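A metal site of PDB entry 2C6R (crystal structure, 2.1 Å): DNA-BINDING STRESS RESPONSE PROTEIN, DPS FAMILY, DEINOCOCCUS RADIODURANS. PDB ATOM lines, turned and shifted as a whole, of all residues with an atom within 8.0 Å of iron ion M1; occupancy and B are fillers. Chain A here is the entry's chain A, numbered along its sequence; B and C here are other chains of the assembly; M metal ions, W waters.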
ATOM      1  N   SER A  93      20.141   7.845   9.272  1.00  0.00           N
ATOM      2  CA  SER A  93      19.358   8.536   8.227  1.00  0.00           C
ATOM      3  C   SER A  93      20.031   8.459   6.837  1.00  0.00           C
ATOM      4  O   SER A  93      19.384   8.243   5.813  1.00  0.00           O
ATOM      5  CB  SER A  93      19.133  10.009   8.594  1.00  0.00           C
ATOM      6  OG  SER A  93      18.406  10.117   9.825  1.00  0.00           O
ATOM      7  N   LYS A  94      21.352   8.640   6.824  1.00  0.00           N
ATOM      8  CA  LYS A  94      22.117   8.627   5.570  1.00  0.00           C
ATOM      9  C   LYS A  94      22.007   7.238   4.919  1.00  0.00           C
ATOM     10  O   LYS A  94      21.777   7.141   3.732  1.00  0.00           O
ATOM     11  CB  LYS A  94      23.581   8.976   5.882  1.00  0.00           C
ATOM     12  CG  LYS A  94      24.612   8.785   4.739  1.00  0.00           C
ATOM     13  CD  LYS A  94      26.056   8.995   5.291  1.00  0.00           C
ATOM     14  CE  LYS A  94      27.061   7.969   4.747  1.00  0.00           C
ATOM     15  NZ  LYS A  94      26.686   7.581   3.355  1.00  0.00           N
ATOM     16  N   ALA A  96      19.670   4.946   5.525  1.00  0.00           N
ATOM     17  CA  ALA A  96      18.260   4.699   5.178  1.00  0.00           C
ATOM     18  C   ALA A  96      17.984   5.227   3.764  1.00  0.00           C
ATOM     19  O   ALA A  96      17.340   4.533   2.931  1.00  0.00           O
ATOM     20  CB  ALA A  96      17.323   5.349   6.196  1.00  0.00           C
ATOM     21  N   ASP A  97      18.472   6.440   3.497  1.00  0.00           N
ATOM     22  CA  ASP A  97      18.366   7.009   2.161  1.00  0.00           C
ATOM     23  C   ASP A  97      19.115   6.181   1.089  1.00  0.00           C
ATOM     24  O   ASP A  97      18.597   5.980  -0.030  1.00  0.00           O
ATOM     25  CB  ASP A  97      18.750   8.499   2.135  1.00  0.00           C
ATOM     26  CG  ASP A  97      18.327   9.171   0.857  1.00  0.00           C
ATOM     27  OD1 ASP A  97      17.131   9.495   0.702  1.00  0.00           O
ATOM     28  OD2 ASP A  97      19.193   9.350  -0.021  1.00  0.00           O
ATOM     29  N   ASP A  98      20.305   5.691   1.420  1.00  0.00           N
ATOM     30  CA  ASP A  98      21.069   4.821   0.474  1.00  0.00           C
ATOM     31  C   ASP A  98      20.387   3.480   0.198  1.00  0.00           C
ATOM     32  O   ASP A  98      20.392   3.005  -0.936  1.00  0.00           O
ATOM     33  CB  ASP A  98      22.494   4.538   1.007  1.00  0.00           C
ATOM     34  CG  ASP A  98      23.388   5.785   0.960  1.00  0.00           C
ATOM     35  OD1 ASP A  98      23.127   6.668   0.146  1.00  0.00           O
ATOM     36  OD2 ASP A  98      24.342   5.875   1.734  1.00  0.00           O
ATOM     37  N   ALA A 100      17.073   2.737   0.606  1.00  0.00           N
ATOM     38  CA  ALA A 100      15.874   3.029  -0.201  1.00  0.00           C
ATOM     39  C   ALA A 100      16.198   3.286  -1.666  1.00  0.00           C
ATOM     40  O   ALA A 100      15.516   2.772  -2.563  1.00  0.00           O
ATOM     41  CB  ALA A 100      15.097   4.183   0.404  1.00  0.00           C
ATOM     42  N   GLU A 101      17.254   4.051  -1.932  1.00  0.00           N
ATOM     43  CA  GLU A 101      17.605   4.331  -3.328  1.00  0.00           C
ATOM     44  C   GLU A 101      18.336   3.178  -4.007  1.00  0.00           C
ATOM     45  O   GLU A 101      18.279   3.065  -5.211  1.00  0.00           O
ATOM     46  CB  GLU A 101      18.307   5.694  -3.479  1.00  0.00           C
ATOM     47  CG  GLU A 101      17.332   6.841  -3.051  1.00  0.00           C
ATOM     48  CD  GLU A 101      17.908   8.216  -3.019  1.00  0.00           C
ATOM     49  OE1 GLU A 101      19.110   8.389  -3.347  1.00  0.00           O
ATOM     50  OE2 GLU A 101      17.148   9.151  -2.671  1.00  0.00           O
ATOM     51  N   LYS B  67       9.793  11.906   2.318  1.00  0.00           N
ATOM     52  CA  LYS B  67      10.847  10.955   1.967  1.00  0.00           C
ATOM     53  C   LYS B  67      10.288   9.870   1.028  1.00  0.00           C
ATOM     54  O   LYS B  67      10.923   9.514   0.039  1.00  0.00           O
ATOM     55  CB  LYS B  67      11.388  10.223   3.187  1.00  0.00           C
ATOM     56  CG  LYS B  67      12.711  10.695   3.737  1.00  0.00           C
ATOM     57  CD  LYS B  67      13.806  10.888   2.708  1.00  0.00           C
ATOM     58  CE  LYS B  67      14.960  11.540   3.416  1.00  0.00           C
ATOM     59  NZ  LYS B  67      16.128  11.482   2.571  1.00  0.00           N
ATOM     60  N   HIS B  70       9.912  11.343  -2.209  1.00  0.00           N
ATOM     61  CA  HIS B  70      11.296  11.595  -2.682  1.00  0.00           C
ATOM     62  C   HIS B  70      11.841  10.349  -3.402  1.00  0.00           C
ATOM     63  O   HIS B  70      12.380  10.443  -4.533  1.00  0.00           O
ATOM     64  CB  HIS B  70      12.145  11.994  -1.446  1.00  0.00           C
ATOM     65  CG  HIS B  70      13.624  12.042  -1.667  1.00  0.00           C
ATOM     66  ND1 HIS B  70      14.256  13.077  -2.313  1.00  0.00           N
ATOM     67  CD2 HIS B  70      14.610  11.212  -1.240  1.00  0.00           C
ATOM     68  CE1 HIS B  70      15.555  12.879  -2.324  1.00  0.00           C
ATOM     69  NE2 HIS B  70      15.796  11.762  -1.662  1.00  0.00           N
ATOM     70  N   TRP B  71      11.689   9.186  -2.760  1.00  0.00           N
ATOM     71  CA  TRP B  71      12.136   7.913  -3.352  1.00  0.00           C
ATOM     72  C   TRP B  71      11.336   7.422  -4.568  1.00  0.00           C
ATOM     73  O   TRP B  71      11.929   6.955  -5.550  1.00  0.00           O
ATOM     74  CB  TRP B  71      12.221   6.791  -2.298  1.00  0.00           C
ATOM     75  CG  TRP B  71      13.134   7.072  -1.108  1.00  0.00           C
ATOM     76  CD1 TRP B  71      14.387   7.648  -1.129  1.00  0.00           C
ATOM     77  CD2 TRP B  71      12.876   6.745   0.266  1.00  0.00           C
ATOM     78  NE1 TRP B  71      14.884   7.741   0.135  1.00  0.00           N
ATOM     79  CE2 TRP B  71      13.989   7.177   1.016  1.00  0.00           C
ATOM     80  CE3 TRP B  71      11.785   6.108   0.937  1.00  0.00           C
ATOM     81  CZ2 TRP B  71      14.079   7.012   2.424  1.00  0.00           C
ATOM     82  CZ3 TRP B  71      11.847   5.967   2.352  1.00  0.00           C
ATOM     83  CH2 TRP B  71      12.993   6.414   3.076  1.00  0.00           C
ATOM     84  N   HIS B  82      11.838  15.143  -6.641  1.00  0.00           N
ATOM     85  CA  HIS B  82      12.841  14.487  -5.815  1.00  0.00           C
ATOM     86  C   HIS B  82      13.694  15.523  -5.056  1.00  0.00           C
ATOM     87  O   HIS B  82      13.902  15.402  -3.850  1.00  0.00           O
ATOM     88  CB  HIS B  82      13.681  13.567  -6.716  1.00  0.00           C
ATOM     89  CG  HIS B  82      14.794  12.830  -6.040  1.00  0.00           C
ATOM     90  ND1 HIS B  82      14.594  11.721  -5.239  1.00  0.00           N
ATOM     91  CD2 HIS B  82      16.149  12.961  -6.158  1.00  0.00           C
ATOM     92  CE1 HIS B  82      15.772  11.226  -4.873  1.00  0.00           C
ATOM     93  NE2 HIS B  82      16.722  11.960  -5.418  1.00  0.00           N
ATOM     94  N   GLU B  83      14.164  16.541  -5.779  1.00  0.00           N
ATOM     95  CA  GLU B  83      14.981  17.633  -5.188  1.00  0.00           C
ATOM     96  C   GLU B  83      14.140  18.553  -4.288  1.00  0.00           C
ATOM     97  O   GLU B  83      14.540  18.867  -3.149  1.00  0.00           O
ATOM     98  CB  GLU B  83      15.633  18.485  -6.303  1.00  0.00           C
ATOM     99  CG  GLU B  83      16.661  17.744  -7.195  1.00  0.00           C
ATOM    100  CD  GLU B  83      17.783  17.149  -6.377  1.00  0.00           C
ATOM    101  OE1 GLU B  83      18.583  17.916  -5.801  1.00  0.00           O
ATOM    102  OE2 GLU B  83      17.881  15.902  -6.264  1.00  0.00           O
ATOM    103  N   GLN B  86      13.246  16.816  -1.080  1.00  0.00           N
ATOM    104  CA  GLN B  86      14.406  16.754  -0.159  1.00  0.00           C
ATOM    105  C   GLN B  86      14.537  18.055   0.654  1.00  0.00           C
ATOM    106  O   GLN B  86      14.771  18.019   1.864  1.00  0.00           O
ATOM    107  CB  GLN B  86      15.698  16.383  -0.896  1.00  0.00           C
ATOM    108  CG  GLN B  86      16.967  16.230  -0.018  1.00  0.00           C
ATOM    109  CD  GLN B  86      16.796  15.243   1.129  1.00  0.00           C
ATOM    110  OE1 GLN B  86      16.117  14.207   1.001  1.00  0.00           O
ATOM    111  NE2 GLN B  86      17.432  15.544   2.256  1.00  0.00           N
ATOM    112  N   LYS C 178      22.382   3.448  -9.950  1.00  0.00           N
ATOM    113  CA  LYS C 178      21.631   4.585  -9.389  1.00  0.00           C
ATOM    114  C   LYS C 178      21.274   5.595 -10.483  1.00  0.00           C
ATOM    115  O   LYS C 178      20.139   6.069 -10.562  1.00  0.00           O
ATOM    116  CB  LYS C 178      22.434   5.260  -8.267  1.00  0.00           C
ATOM    117  CG  LYS C 178      21.778   6.522  -7.670  1.00  0.00           C
ATOM    118  CD  LYS C 178      22.600   6.958  -6.480  1.00  0.00           C
ATOM    119  CE  LYS C 178      22.109   8.260  -5.919  1.00  0.00           C
ATOM    120  NZ  LYS C 178      22.984   8.564  -4.755  1.00  0.00           N
ATOM    121  N   TRP C 181      18.391   4.278 -12.627  1.00  0.00           N
ATOM    122  CA  TRP C 181      17.110   4.573 -12.007  1.00  0.00           C
ATOM    123  C   TRP C 181      16.728   6.052 -12.238  1.00  0.00           C
ATOM    124  O   TRP C 181      15.592   6.370 -12.564  1.00  0.00           O
ATOM    125  CB  TRP C 181      17.147   4.209 -10.502  1.00  0.00           C
ATOM    126  CG  TRP C 181      16.221   5.101  -9.664  1.00  0.00           C
ATOM    127  CD1 TRP C 181      14.874   5.241  -9.798  1.00  0.00           C
ATOM    128  CD2 TRP C 181      16.610   5.950  -8.589  1.00  0.00           C
ATOM    129  NE1 TRP C 181      14.387   6.144  -8.872  1.00  0.00           N
ATOM    130  CE2 TRP C 181      15.431   6.575  -8.094  1.00  0.00           C
ATOM    131  CE3 TRP C 181      17.830   6.214  -7.955  1.00  0.00           C
ATOM    132  CZ2 TRP C 181      15.453   7.485  -7.024  1.00  0.00           C
ATOM    133  CZ3 TRP C 181      17.848   7.143  -6.895  1.00  0.00           C
ATOM    134  CH2 TRP C 181      16.658   7.734  -6.440  1.00  0.00           C
ATOM    135  N   GLN C 182      17.695   6.955 -12.076  1.00  0.00           N
ATOM    136  CA  GLN C 182      17.396   8.381 -12.203  1.00  0.00           C
ATOM    137  C   GLN C 182      16.933   8.743 -13.630  1.00  0.00           C
ATOM    138  O   GLN C 182      16.184   9.691 -13.809  1.00  0.00           O
ATOM    139  CB  GLN C 182      18.594   9.247 -11.724  1.00  0.00           C
ATOM    140  CG  GLN C 182      18.878   9.101 -10.214  1.00  0.00           C
ATOM    141  CD  GLN C 182      19.994   9.988  -9.699  1.00  0.00           C
ATOM    142  OE1 GLN C 182      20.921  10.360 -10.432  1.00  0.00           O
ATOM    143  NE2 GLN C 182      19.917  10.344  -8.409  1.00  0.00           N
HETATM  144 FE    FE M   1      17.684  10.642  -1.312  1.00  0.00          FE
HETATM  145 FE    FE M   2      23.405   9.031   0.210  1.00  0.00          FE
HETATM  146  O   HOH W   1      18.147  12.164   0.283  1.00  0.00           O
HETATM  147  O   HOH W   2      18.956  11.658  -2.939  1.00  0.00           O
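Iron ion M1 is bound by OE2 of Glu 101, NE2 of His 70 of chain B, water W1, water W2, OD2 of Asp 97 and OD1 of Asp 97.
Iron ion M1 has six donor atoms within binding distance.
The side-chain carboxylate of Asp 97 sits close to the indole nitrogen of Trp 71 of chain B.
The backbone carbonyl oxygen of His 70 of chain B is in hydrogen-bond range of a ring nitrogen (ND1) of His 82 of chain B (2.7 Å).
OD1 of Asp 97 sits close to NZ of Lys 67 of chain B (2.9 Å).
Three residues have an atom within 4 Å of iron ion M1: Asp 97, Glu 101 and His 70 of chain B.
Water W1 bridges the side-chain amide oxygen of Gln 86 of chain B (3.0 Å) and the side-chain amino group of Lys 67 of chain B (3.1 Å).
Water W2 bridges the side-chain carboxylate (OE1) of Glu 101 (3.3 Å) and a ring nitrogen (NE2) of His 82 of chain B (3.4 Å).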
